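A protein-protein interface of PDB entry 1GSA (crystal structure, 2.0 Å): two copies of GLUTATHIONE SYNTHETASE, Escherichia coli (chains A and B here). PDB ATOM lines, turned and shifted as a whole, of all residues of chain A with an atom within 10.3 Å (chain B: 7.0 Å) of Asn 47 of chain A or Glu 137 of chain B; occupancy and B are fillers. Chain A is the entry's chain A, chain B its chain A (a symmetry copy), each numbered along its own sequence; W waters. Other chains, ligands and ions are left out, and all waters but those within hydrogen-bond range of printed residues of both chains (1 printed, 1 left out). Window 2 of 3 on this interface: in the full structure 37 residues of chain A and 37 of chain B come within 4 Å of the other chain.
ND2 of Asn 47 of chain A is in hydrogen-bond range of OE1 of Glu 137 of chain B, at 3.5 Å. NH2 of Arg 104 of chain A sits at hydrogen-bond distance from O of Ala 129 of chain B, at 3.3 Å. The backbone NH (N) of Asn 47 of chain A is in hydrogen-bond range of the backbone carbonyl oxygen (O) of Thr 138 of chain B, 2.9 Å away. N of Val 140 of chain B lies within hydrogen-bond range of O of Leu 45 of chain A, at 2.8 Å.
CD1 of Leu 139 of chain B touches CD2 of Tyr 44 of chain A, at 3.9 Å. Tyr 44 of chain A touches Val 140 of chain B (CB to O, 3.2 Å). O of Thr 138 of chain B touches O of Leu 45 of chain A (3.7 Å). O of Leu 45 of chain A touches CA of Leu 139 of chain B, at 3.2 Å. Ile 46 of chain A touches Thr 138 of chain B. Asn 47 of chain A touches Ser 132 of chain B. Asn 47 of chain A touches Pro 136 of chain B (OD1 to O, 3.8 Å). CA of Gly 48 of chain A touches O of Ala 129 of chain B, 3.7 Å away.
Water W1 lies within hydrogen-bond range of N of Gly 48 of chain A (2.9 Å), O of Thr 138 of chain B (2.9 Å) and N of Asn 47 of chain A (3.0 Å).
No position is printed for both chains. Of the 12 pairs that touch across the chains among the printed residues, none has its exchanged pair printed and touching as well.
The side-chain hydroxyl of Thr 135 of chain B lies close to the backbone carbonyl oxygen of Ser 132 of chain B, 3.5 Å away. O of Tyr 44 of chain A is in hydrogen-bond range of N of Arg 51 of chain A (3.0 Å). The side-chain carboxylate (OE1) of Glu 137 of chain B lies within salt-bridge range of the side-chain amino group (NZ) of Lys 153 of chain B, at 3.7 Å. The backbone NH (N) of Glu 137 of chain B lies within hydrogen-bond range of the side-chain amide oxygen (OD1) of Asn 199 of chain B, at 2.7 Å. OE1 of Glu 107 of chain A is in salt-bridge range of NH1 of Arg 104 of chain A, 2.7 Å away. The side-chain hydroxyl (OG1) of Thr 138 of chain B sits at hydrogen-bond distance from the backbone carbonyl oxygen (O) of Pro 136 of chain B (3.0 Å).
Hydrophobic or aromatic side chains of chain A that line the printed part of chain B: Tyr 44, Leu 45 and Ile 46. Of the 22 printed residues of chain B, 7 touch a printed residue of chain A. Printed residues of chain B that touch a printed residue of chain A: Ala 129, Ser 132, Pro 136, Glu 137, Thr 138, Leu 139 and Val 140. Among the printed residues, no Asp or Glu carboxylate lies within 4 Å of a Lys or Arg side-chain nitrogen of the other chain.
Printed residues of chain B within 4 Å of Leu 45 of chain A: Thr 138, Leu 139 and Val 140. Of chain B, only Ser 132 (3.3 Å), Pro 136 (3.8 Å), Glu 137 (3.2 Å) and Thr 138 (2.9 Å) come within 4 Å of Asn 47 of chain A. Of the printed residues of chain B, Gly 48 of chain A touches Ala 129 (3.7 Å). Arg 51 of chain A touches none of the printed residues of chain B. Of the printed residues of chain B, Arg 104 of chain A touches Ala 129 (3.3 Å). Of chain A, only Asn 47 comes within 4 Å of Ser 132 of chain B. Of chain A, only Asn 47 (3.8 Å) comes within 4 Å of Pro 136 of chain B. Glu 137 of chain B touches one residue of chain A. Of chain A, only Leu 45, Ile 46 and Asn 47 come within 4 Å of Thr 138 of chain B. Of the printed residues of chain A, Leu 139 of chain B touches Tyr 44 and Leu 45. The nearest printed residue of chain B that does not touch Asn 47 of chain A is Ala 129 of chain B (5.0 Å). The nearest residue of chain A that does not touch Glu 137 of chain B is Ile 46 of chain A (5.1 Å).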
ATOM      1  N   TYR A  44     -35.302 -18.374 -24.754  1.00  0.00           N
ATOM      2  CA  TYR A  44     -34.286 -17.596 -25.397  1.00  0.00           C
ATOM      3  C   TYR A  44     -33.216 -18.516 -25.930  1.00  0.00           C
ATOM      4  O   TYR A  44     -33.232 -19.727 -25.694  1.00  0.00           O
ATOM      5  CB  TYR A  44     -33.710 -16.591 -24.396  1.00  0.00           C
ATOM      6  CG  TYR A  44     -32.958 -17.108 -23.193  1.00  0.00           C
ATOM      7  CD1 TYR A  44     -33.621 -17.510 -22.029  1.00  0.00           C
ATOM      8  CD2 TYR A  44     -31.564 -17.136 -23.273  1.00  0.00           C
ATOM      9  CE1 TYR A  44     -32.863 -17.929 -20.930  1.00  0.00           C
ATOM     10  CE2 TYR A  44     -30.812 -17.548 -22.177  1.00  0.00           C
ATOM     11  CZ  TYR A  44     -31.462 -17.936 -21.018  1.00  0.00           C
ATOM     12  OH  TYR A  44     -30.677 -18.312 -19.951  1.00  0.00           O
ATOM     13  N   LEU A  45     -32.299 -17.911 -26.667  1.00  0.00           N
ATOM     14  CA  LEU A  45     -31.185 -18.594 -27.290  1.00  0.00           C
ATOM     15  C   LEU A  45     -29.956 -17.794 -26.925  1.00  0.00           C
ATOM     16  O   LEU A  45     -29.976 -16.574 -27.081  1.00  0.00           O
ATOM     17  CB  LEU A  45     -31.233 -18.607 -28.820  1.00  0.00           C
ATOM     18  CG  LEU A  45     -32.035 -19.633 -29.571  1.00  0.00           C
ATOM     19  CD1 LEU A  45     -31.828 -19.415 -31.063  1.00  0.00           C
ATOM     20  CD2 LEU A  45     -31.594 -21.018 -29.204  1.00  0.00           C
ATOM     21  N   ILE A  46     -28.931 -18.476 -26.388  1.00  0.00           N
ATOM     22  CA  ILE A  46     -27.639 -17.885 -26.067  1.00  0.00           C
ATOM     23  C   ILE A  46     -26.650 -18.850 -26.688  1.00  0.00           C
ATOM     24  O   ILE A  46     -26.560 -20.039 -26.390  1.00  0.00           O
ATOM     25  CB  ILE A  46     -27.470 -17.742 -24.514  1.00  0.00           C
ATOM     26  CG1 ILE A  46     -26.069 -17.195 -24.209  1.00  0.00           C
ATOM     27  CG2 ILE A  46     -27.741 -19.049 -23.819  1.00  0.00           C
ATOM     28  CD1 ILE A  46     -25.693 -15.797 -24.828  1.00  0.00           C
ATOM     29  N   ASN A  47     -26.021 -18.346 -27.731  1.00  0.00           N
ATOM     30  CA  ASN A  47     -25.054 -19.058 -28.549  1.00  0.00           C
ATOM     31  C   ASN A  47     -25.574 -20.397 -29.037  1.00  0.00           C
ATOM     32  O   ASN A  47     -24.932 -21.445 -28.936  1.00  0.00           O
ATOM     33  CB  ASN A  47     -23.782 -19.289 -27.783  1.00  0.00           C
ATOM     34  CG  ASN A  47     -23.102 -17.993 -27.432  1.00  0.00           C
ATOM     35  OD1 ASN A  47     -22.991 -17.048 -28.215  1.00  0.00           O
ATOM     36  ND2 ASN A  47     -22.641 -17.901 -26.209  1.00  0.00           N
ATOM     37  N   GLY A  48     -26.819 -20.372 -29.494  1.00  0.00           N
ATOM     38  CA  GLY A  48     -27.460 -21.524 -30.081  1.00  0.00           C
ATOM     39  C   GLY A  48     -27.943 -22.521 -29.072  1.00  0.00           C
ATOM     40  O   GLY A  48     -28.405 -23.573 -29.481  1.00  0.00           O
ATOM     41  N   GLU A  49     -27.847 -22.265 -27.771  1.00  0.00           N
ATOM     42  CA  GLU A  49     -28.357 -23.162 -26.756  1.00  0.00           C
ATOM     43  C   GLU A  49     -29.722 -22.593 -26.384  1.00  0.00           C
ATOM     44  O   GLU A  49     -29.845 -21.407 -26.071  1.00  0.00           O
ATOM     45  CB  GLU A  49     -27.451 -23.147 -25.569  1.00  0.00           C
ATOM     46  CG  GLU A  49     -27.849 -24.170 -24.533  1.00  0.00           C
ATOM     47  CD  GLU A  49     -27.262 -23.995 -23.131  1.00  0.00           C
ATOM     48  OE1 GLU A  49     -26.731 -22.951 -22.755  1.00  0.00           O
ATOM     49  OE2 GLU A  49     -27.365 -24.924 -22.356  1.00  0.00           O
ATOM     50  N   ALA A  50     -30.763 -23.399 -26.494  1.00  0.00           N
ATOM     51  CA  ALA A  50     -32.114 -23.013 -26.152  1.00  0.00           C
ATOM     52  C   ALA A  50     -32.216 -23.149 -24.647  1.00  0.00           C
ATOM     53  O   ALA A  50     -31.883 -24.214 -24.106  1.00  0.00           O
ATOM     54  CB  ALA A  50     -33.123 -23.954 -26.789  1.00  0.00           C
ATOM     55  N   ARG A  51     -32.691 -22.121 -23.979  1.00  0.00           N
ATOM     56  CA  ARG A  51     -32.811 -22.127 -22.548  1.00  0.00           C
ATOM     57  C   ARG A  51     -34.104 -21.437 -22.192  1.00  0.00           C
ATOM     58  O   ARG A  51     -34.680 -20.787 -23.056  1.00  0.00           O
ATOM     59  CB  ARG A  51     -31.665 -21.367 -21.908  1.00  0.00           C
ATOM     60  CG  ARG A  51     -30.262 -21.900 -22.139  1.00  0.00           C
ATOM     61  CD  ARG A  51     -29.250 -21.053 -21.380  1.00  0.00           C
ATOM     62  NE  ARG A  51     -29.371 -21.273 -19.956  1.00  0.00           N
ATOM     63  CZ  ARG A  51     -28.831 -22.338 -19.363  1.00  0.00           C
ATOM     64  NH1 ARG A  51     -28.138 -23.262 -20.021  1.00  0.00           N
ATOM     65  NH2 ARG A  51     -29.045 -22.536 -18.078  1.00  0.00           N
ATOM     66  N   ILE A 101     -36.202 -22.089 -31.676  1.00  0.00           N
ATOM     67  CA  ILE A 101     -35.735 -22.222 -30.302  1.00  0.00           C
ATOM     68  C   ILE A 101     -36.159 -23.592 -29.833  1.00  0.00           C
ATOM     69  O   ILE A 101     -35.338 -24.346 -29.313  1.00  0.00           O
ATOM     70  CB  ILE A 101     -36.346 -21.115 -29.429  1.00  0.00           C
ATOM     71  CG1 ILE A 101     -35.778 -19.791 -29.908  1.00  0.00           C
ATOM     72  CG2 ILE A 101     -36.105 -21.397 -27.953  1.00  0.00           C
ATOM     73  CD1 ILE A 101     -36.542 -18.612 -29.328  1.00  0.00           C
ATOM     74  N   ARG A 104     -33.762 -26.264 -31.296  1.00  0.00           N
ATOM     75  CA  ARG A 104     -32.419 -26.480 -30.755  1.00  0.00           C
ATOM     76  C   ARG A 104     -32.440 -27.427 -29.549  1.00  0.00           C
ATOM     77  O   ARG A 104     -31.488 -28.171 -29.307  1.00  0.00           O
ATOM     78  CB  ARG A 104     -31.822 -25.125 -30.374  1.00  0.00           C
ATOM     79  CG  ARG A 104     -31.564 -24.247 -31.580  1.00  0.00           C
ATOM     80  CD  ARG A 104     -30.533 -24.900 -32.496  1.00  0.00           C
ATOM     81  NE  ARG A 104     -29.222 -24.751 -31.915  1.00  0.00           N
ATOM     82  CZ  ARG A 104     -28.185 -25.522 -32.200  1.00  0.00           C
ATOM     83  NH1 ARG A 104     -28.221 -26.503 -33.060  1.00  0.00           N
ATOM     84  NH2 ARG A 104     -27.091 -25.383 -31.497  1.00  0.00           N
ATOM     85  N   GLU A 107     -32.925 -31.034 -30.969  1.00  0.00           N
ATOM     86  CA  GLU A 107     -31.689 -31.686 -31.383  1.00  0.00           C
ATOM     87  C   GLU A 107     -30.880 -32.232 -30.219  1.00  0.00           C
ATOM     88  O   GLU A 107     -30.058 -33.123 -30.394  1.00  0.00           O
ATOM     89  CB  GLU A 107     -30.803 -30.747 -32.105  1.00  0.00           C
ATOM     90  CG  GLU A 107     -31.235 -30.507 -33.531  1.00  0.00           C
ATOM     91  CD  GLU A 107     -30.679 -29.202 -34.068  1.00  0.00           C
ATOM     92  OE1 GLU A 107     -29.722 -28.659 -33.494  1.00  0.00           O
ATOM     93  OE2 GLU A 107     -31.230 -28.742 -35.071  1.00  0.00           O
ATOM     94  N   LYS A 108     -31.072 -31.718 -29.019  1.00  0.00           N
ATOM     95  CA  LYS A 108     -30.409 -32.235 -27.862  1.00  0.00           C
ATOM     96  C   LYS A 108     -31.239 -33.348 -27.277  1.00  0.00           C
ATOM     97  O   LYS A 108     -30.960 -33.765 -26.165  1.00  0.00           O
ATOM     98  CB  LYS A 108     -30.234 -31.094 -26.894  1.00  0.00           C
ATOM     99  CG  LYS A 108     -29.364 -30.016 -27.487  1.00  0.00           C
ATOM    100  CD  LYS A 108     -27.950 -30.557 -27.426  1.00  0.00           C
ATOM    101  CE  LYS A 108     -27.101 -30.222 -28.663  1.00  0.00           C
ATOM    102  NZ  LYS A 108     -26.621 -28.849 -28.667  1.00  0.00           N
ATOM    103  N   THR B 128     -27.744 -18.889 -37.786  1.00  0.00           N
ATOM    104  CA  THR B 128     -26.413 -18.777 -37.208  1.00  0.00           C
ATOM    105  C   THR B 128     -26.335 -19.594 -35.935  1.00  0.00           C
ATOM    106  O   THR B 128     -25.247 -20.011 -35.559  1.00  0.00           O
ATOM    107  CB  THR B 128     -26.082 -17.315 -36.867  1.00  0.00           C
ATOM    108  OG1 THR B 128     -27.065 -16.850 -35.944  1.00  0.00           O
ATOM    109  CG2 THR B 128     -26.050 -16.455 -38.098  1.00  0.00           C
ATOM    110  N   ALA B 129     -27.457 -19.850 -35.258  1.00  0.00           N
ATOM    111  CA  ALA B 129     -27.545 -20.704 -34.091  1.00  0.00           C
ATOM    112  C   ALA B 129     -27.065 -22.114 -34.380  1.00  0.00           C
ATOM    113  O   ALA B 129     -26.638 -22.823 -33.471  1.00  0.00           O
ATOM    114  CB  ALA B 129     -28.978 -20.783 -33.611  1.00  0.00           C
ATOM    115  N   PHE B 131     -24.336 -22.686 -36.052  1.00  0.00           N
ATOM    116  CA  PHE B 131     -22.887 -22.594 -36.266  1.00  0.00           C
ATOM    117  C   PHE B 131     -22.324 -21.617 -35.233  1.00  0.00           C
ATOM    118  O   PHE B 131     -21.508 -20.755 -35.556  1.00  0.00           O
ATOM    119  CB  PHE B 131     -22.570 -22.062 -37.662  1.00  0.00           C
ATOM    120  CG  PHE B 131     -23.216 -22.858 -38.791  1.00  0.00           C
ATOM    121  CD1 PHE B 131     -22.627 -24.046 -39.243  1.00  0.00           C
ATOM    122  CD2 PHE B 131     -24.412 -22.400 -39.363  1.00  0.00           C
ATOM    123  CE1 PHE B 131     -23.244 -24.767 -40.262  1.00  0.00           C
ATOM    124  CE2 PHE B 131     -25.016 -23.140 -40.386  1.00  0.00           C
ATOM    125  CZ  PHE B 131     -24.434 -24.318 -40.832  1.00  0.00           C
ATOM    126  N   SER B 132     -22.692 -21.750 -33.961  1.00  0.00           N
ATOM    127  CA  SER B 132     -22.316 -20.811 -32.905  1.00  0.00           C
ATOM    128  C   SER B 132     -20.832 -20.727 -32.610  1.00  0.00           C
ATOM    129  O   SER B 132     -20.319 -19.834 -31.942  1.00  0.00           O
ATOM    130  CB  SER B 132     -23.017 -21.184 -31.640  1.00  0.00           C
ATOM    131  OG  SER B 132     -22.653 -22.527 -31.386  1.00  0.00           O
ATOM    132  N   ASP B 133     -20.109 -21.726 -33.081  1.00  0.00           N
ATOM    133  CA  ASP B 133     -18.649 -21.736 -33.047  1.00  0.00           C
ATOM    134  C   ASP B 133     -18.018 -20.757 -34.056  1.00  0.00           C
ATOM    135  O   ASP B 133     -16.817 -20.478 -34.010  1.00  0.00           O
ATOM    136  CB  ASP B 133     -18.142 -23.193 -33.311  1.00  0.00           C
ATOM    137  CG  ASP B 133     -18.765 -23.905 -34.531  1.00  0.00           C
ATOM    138  OD1 ASP B 133     -19.980 -24.177 -34.524  1.00  0.00           O
ATOM    139  OD2 ASP B 133     -18.029 -24.184 -35.490  1.00  0.00           O
ATOM    140  N   THR B 135     -19.868 -17.765 -34.984  1.00  0.00           N
ATOM    141  CA  THR B 135     -20.542 -16.457 -34.875  1.00  0.00           C
ATOM    142  C   THR B 135     -20.049 -15.592 -33.731  1.00  0.00           C
ATOM    143  O   THR B 135     -19.298 -16.142 -32.925  1.00  0.00           O
ATOM    144  CB  THR B 135     -22.060 -16.698 -34.730  1.00  0.00           C
ATOM    145  OG1 THR B 135     -22.334 -17.473 -33.552  1.00  0.00           O
ATOM    146  CG2 THR B 135     -22.563 -17.474 -35.928  1.00  0.00           C
ATOM    147  N   PRO B 136     -20.364 -14.307 -33.504  1.00  0.00           N
ATOM    148  CA  PRO B 136     -20.119 -13.691 -32.206  1.00  0.00           C
ATOM    149  C   PRO B 136     -21.034 -14.240 -31.124  1.00  0.00           C
ATOM    150  O   PRO B 136     -21.813 -15.188 -31.352  1.00  0.00           O
ATOM    151  CB  PRO B 136     -20.283 -12.229 -32.478  1.00  0.00           C
ATOM    152  CG  PRO B 136     -21.105 -12.142 -33.730  1.00  0.00           C
ATOM    153  CD  PRO B 136     -20.693 -13.334 -34.539  1.00  0.00           C
ATOM    154  N   GLU B 137     -20.905 -13.739 -29.899  1.00  0.00           N
ATOM    155  CA  GLU B 137     -21.782 -14.090 -28.781  1.00  0.00           C
ATOM    156  C   GLU B 137     -23.156 -13.612 -29.225  1.00  0.00           C
ATOM    157  O   GLU B 137     -23.264 -12.442 -29.595  1.00  0.00           O
ATOM    158  CB  GLU B 137     -21.443 -13.333 -27.503  1.00  0.00           C
ATOM    159  CG  GLU B 137     -20.070 -13.597 -26.961  1.00  0.00           C
ATOM    160  CD  GLU B 137     -19.927 -14.923 -26.254  1.00  0.00           C
ATOM    161  OE1 GLU B 137     -20.640 -15.202 -25.285  1.00  0.00           O
ATOM    162  OE2 GLU B 137     -19.058 -15.670 -26.684  1.00  0.00           O
ATOM    163  N   THR B 138     -24.183 -14.455 -29.222  1.00  0.00           N
ATOM    164  CA  THR B 138     -25.489 -14.064 -29.719  1.00  0.00           C
ATOM    165  C   THR B 138     -26.570 -14.465 -28.752  1.00  0.00           C
ATOM    166  O   THR B 138     -26.648 -15.625 -28.352  1.00  0.00           O
ATOM    167  CB  THR B 138     -25.727 -14.734 -31.037  1.00  0.00           C
ATOM    168  OG1 THR B 138     -24.656 -14.437 -31.905  1.00  0.00           O
ATOM    169  CG2 THR B 138     -26.957 -14.210 -31.691  1.00  0.00           C
ATOM    170  N   LEU B 139     -27.458 -13.540 -28.425  1.00  0.00           N
ATOM    171  CA  LEU B 139     -28.556 -13.756 -27.525  1.00  0.00           C
ATOM    172  C   LEU B 139     -29.793 -13.391 -28.315  1.00  0.00           C
ATOM    173  O   LEU B 139     -29.789 -12.332 -28.956  1.00  0.00           O
ATOM    174  CB  LEU B 139     -28.418 -12.826 -26.299  1.00  0.00           C
ATOM    175  CG  LEU B 139     -29.525 -12.661 -25.242  1.00  0.00           C
ATOM    176  CD1 LEU B 139     -29.687 -13.909 -24.404  1.00  0.00           C
ATOM    177  CD2 LEU B 139     -29.147 -11.524 -24.309  1.00  0.00           C
ATOM    178  N   VAL B 140     -30.845 -14.211 -28.290  1.00  0.00           N
ATOM    179  CA  VAL B 140     -32.105 -13.884 -28.909  1.00  0.00           C
ATOM    180  C   VAL B 140     -33.071 -13.843 -27.742  1.00  0.00           C
ATOM    181  O   VAL B 140     -33.227 -14.864 -27.085  1.00  0.00           O
ATOM    182  CB  VAL B 140     -32.454 -14.982 -29.940  1.00  0.00           C
ATOM    183  CG1 VAL B 140     -33.855 -14.833 -30.518  1.00  0.00           C
ATOM    184  CG2 VAL B 140     -31.413 -14.874 -31.042  1.00  0.00           C
ATOM    185  N   PHE B 150     -26.416  -8.697 -20.893  1.00  0.00           N
ATOM    186  CA  PHE B 150     -25.482  -8.961 -21.991  1.00  0.00           C
ATOM    187  C   PHE B 150     -24.631  -7.753 -22.343  1.00  0.00           C
ATOM    188  O   PHE B 150     -23.462  -7.870 -22.748  1.00  0.00           O
ATOM    189  CB  PHE B 150     -26.282  -9.402 -23.205  1.00  0.00           C
ATOM    190  CG  PHE B 150     -25.547  -9.981 -24.401  1.00  0.00           C
ATOM    191  CD1 PHE B 150     -25.139 -11.313 -24.411  1.00  0.00           C
ATOM    192  CD2 PHE B 150     -25.302  -9.174 -25.511  1.00  0.00           C
ATOM    193  CE1 PHE B 150     -24.488 -11.834 -25.526  1.00  0.00           C
ATOM    194  CE2 PHE B 150     -24.649  -9.699 -26.628  1.00  0.00           C
ATOM    195  CZ  PHE B 150     -24.246 -11.023 -26.630  1.00  0.00           C
ATOM    196  N   LYS B 153     -21.939  -7.387 -19.493  1.00  0.00           N
ATOM    197  CA  LYS B 153     -20.867  -8.322 -19.757  1.00  0.00           C
ATOM    198  C   LYS B 153     -20.004  -7.890 -20.954  1.00  0.00           C
ATOM    199  O   LYS B 153     -18.784  -8.007 -20.934  1.00  0.00           O
ATOM    200  CB  LYS B 153     -21.454  -9.692 -20.053  1.00  0.00           C
ATOM    201  CG  LYS B 153     -20.418 -10.801 -19.991  1.00  0.00           C
ATOM    202  CD  LYS B 153     -20.837 -12.016 -20.818  1.00  0.00           C
ATOM    203  CE  LYS B 153     -19.775 -13.110 -20.725  1.00  0.00           C
ATOM    204  NZ  LYS B 153     -19.652 -13.837 -21.981  1.00  0.00           N
ATOM    205  N   HIS B 154     -20.569  -7.432 -22.072  1.00  0.00           N
ATOM    206  CA  HIS B 154     -19.789  -7.153 -23.265  1.00  0.00           C
ATOM    207  C   HIS B 154     -19.421  -5.721 -23.562  1.00  0.00           C
ATOM    208  O   HIS B 154     -18.619  -5.514 -24.471  1.00  0.00           O
ATOM    209  CB  HIS B 154     -20.512  -7.718 -24.499  1.00  0.00           C
ATOM    210  CG  HIS B 154     -20.497  -9.234 -24.470  1.00  0.00           C
ATOM    211  ND1 HIS B 154     -19.468 -10.055 -24.670  1.00  0.00           N
ATOM    212  CD2 HIS B 154     -21.595  -9.997 -24.175  1.00  0.00           C
ATOM    213  CE1 HIS B 154     -19.902 -11.274 -24.503  1.00  0.00           C
ATOM    214  NE2 HIS B 154     -21.182 -11.236 -24.212  1.00  0.00           N
ATOM    215  N   ILE B 158     -24.343  -4.889 -30.470  1.00  0.00           N
ATOM    216  CA  ILE B 158     -25.157  -4.644 -31.659  1.00  0.00           C
ATOM    217  C   ILE B 158     -26.503  -5.319 -31.350  1.00  0.00           C
ATOM    218  O   ILE B 158     -26.539  -6.486 -30.944  1.00  0.00           O
ATOM    219  CB  ILE B 158     -24.504  -5.297 -32.899  1.00  0.00           C
ATOM    220  CG1 ILE B 158     -23.243  -4.555 -33.282  1.00  0.00           C
ATOM    221  CG2 ILE B 158     -25.488  -5.317 -34.044  1.00  0.00           C
ATOM    222  CD1 ILE B 158     -23.398  -3.116 -33.779  1.00  0.00           C
ATOM    223  N   MET B 196     -32.299  -9.734 -31.493  1.00  0.00           N
ATOM    224  CA  MET B 196     -31.012 -10.400 -31.393  1.00  0.00           C
ATOM    225  C   MET B 196     -29.972  -9.395 -30.919  1.00  0.00           C
ATOM    226  O   MET B 196     -29.993  -8.261 -31.398  1.00  0.00           O
ATOM    227  CB  MET B 196     -30.638 -10.961 -32.769  1.00  0.00           C
ATOM    228  CG  MET B 196     -29.359 -11.732 -32.687  1.00  0.00           C
ATOM    229  SD  MET B 196     -28.751 -12.287 -34.283  1.00  0.00           S
ATOM    230  CE  MET B 196     -29.431 -13.918 -34.329  1.00  0.00           C
ATOM    231  N   ALA B 197     -29.146  -9.737 -29.932  1.00  0.00           N
ATOM    232  CA  ALA B 197     -28.032  -8.918 -29.488  1.00  0.00           C
ATOM    233  C   ALA B 197     -26.765  -9.677 -29.803  1.00  0.00           C
ATOM    234  O   ALA B 197     -26.766 -10.911 -29.663  1.00  0.00           O
ATOM    235  CB  ALA B 197     -28.011  -8.728 -28.006  1.00  0.00           C
ATOM    236  N   GLN B 198     -25.678  -9.024 -30.199  1.00  0.00           N
ATOM    237  CA  GLN B 198     -24.437  -9.718 -30.481  1.00  0.00           C
ATOM    238  C   GLN B 198     -23.364  -8.808 -29.979  1.00  0.00           C
ATOM    239  O   GLN B 198     -23.569  -7.594 -29.994  1.00  0.00           O
ATOM    240  CB  GLN B 198     -24.059  -9.881 -31.933  1.00  0.00           C
ATOM    241  CG  GLN B 198     -25.017 -10.598 -32.837  1.00  0.00           C
ATOM    242  CD  GLN B 198     -24.387 -10.853 -34.174  1.00  0.00           C
ATOM    243  OE1 GLN B 198     -23.903  -9.960 -34.850  1.00  0.00           O
ATOM    244  NE2 GLN B 198     -24.328 -12.102 -34.575  1.00  0.00           N
ATOM    245  N   ASN B 199     -22.196  -9.301 -29.590  1.00  0.00           N
ATOM    246  CA  ASN B 199     -21.145  -8.370 -29.187  1.00  0.00           C
ATOM    247  C   ASN B 199     -20.600  -7.690 -30.440  1.00  0.00           C
ATOM    248  O   ASN B 199     -20.601  -8.264 -31.524  1.00  0.00           O
ATOM    249  CB  ASN B 199     -19.986  -9.068 -28.426  1.00  0.00           C
ATOM    250  CG  ASN B 199     -19.383 -10.256 -29.125  1.00  0.00           C
ATOM    251  OD1 ASN B 199     -20.054 -11.257 -29.321  1.00  0.00           O
ATOM    252  ND2 ASN B 199     -18.132 -10.299 -29.516  1.00  0.00           N
ATOM    253  N   TYR B 200     -20.245  -6.412 -30.335  1.00  0.00           N
ATOM    254  CA  TYR B 200     -19.776  -5.650 -31.470  1.00  0.00           C
ATOM    255  C   TYR B 200     -18.410  -6.151 -31.898  1.00  0.00           C
ATOM    256  O   TYR B 200     -17.565  -6.466 -31.069  1.00  0.00           O
ATOM    257  CB  TYR B 200     -19.763  -4.190 -31.046  1.00  0.00           C
ATOM    258  CG  TYR B 200     -19.104  -3.217 -32.003  1.00  0.00           C
ATOM    259  CD1 TYR B 200     -19.803  -2.723 -33.106  1.00  0.00           C
ATOM    260  CD2 TYR B 200     -17.767  -2.844 -31.774  1.00  0.00           C
ATOM    261  CE1 TYR B 200     -19.152  -1.859 -33.987  1.00  0.00           C
ATOM    262  CE2 TYR B 200     -17.114  -1.977 -32.648  1.00  0.00           C
ATOM    263  CZ  TYR B 200     -17.807  -1.486 -33.755  1.00  0.00           C
ATOM    264  OH  TYR B 200     -17.153  -0.617 -34.635  1.00  0.00           O
ATOM    265  N   LEU B 201     -18.200  -6.223 -33.199  1.00  0.00           N
ATOM    266  CA  LEU B 201     -16.972  -6.700 -33.794  1.00  0.00           C
ATOM    267  C   LEU B 201     -16.223  -5.538 -34.417  1.00  0.00           C
ATOM    268  O   LEU B 201     -16.590  -5.111 -35.514  1.00  0.00           O
ATOM    269  CB  LEU B 201     -17.279  -7.735 -34.861  1.00  0.00           C
ATOM    270  CG  LEU B 201     -18.008  -8.986 -34.412  1.00  0.00           C
ATOM    271  CD1 LEU B 201     -18.396  -9.788 -35.621  1.00  0.00           C
ATOM    272  CD2 LEU B 201     -17.121  -9.812 -33.520  1.00  0.00           C
ATOM    273  N   ARG B 278     -15.767 -13.743 -37.999  1.00  0.00           N
ATOM    274  CA  ARG B 278     -17.032 -14.198 -37.452  1.00  0.00           C
ATOM    275  C   ARG B 278     -18.099 -14.077 -38.523  1.00  0.00           C
ATOM    276  O   ARG B 278     -18.115 -13.135 -39.330  1.00  0.00           O
ATOM    277  CB  ARG B 278     -17.446 -13.353 -36.277  1.00  0.00           C
ATOM    278  CG  ARG B 278     -16.511 -13.280 -35.082  1.00  0.00           C
ATOM    279  CD  ARG B 278     -16.473 -14.536 -34.259  1.00  0.00           C
ATOM    280  NE  ARG B 278     -15.605 -15.475 -34.908  1.00  0.00           N
ATOM    281  CZ  ARG B 278     -15.570 -16.767 -34.621  1.00  0.00           C
ATOM    282  NH1 ARG B 278     -16.340 -17.338 -33.688  1.00  0.00           N
ATOM    283  NH2 ARG B 278     -14.742 -17.504 -35.349  1.00  0.00           N
HETATM  284  O   HOH W   1     -28.080 -17.752 -29.781  1.00  0.00           O
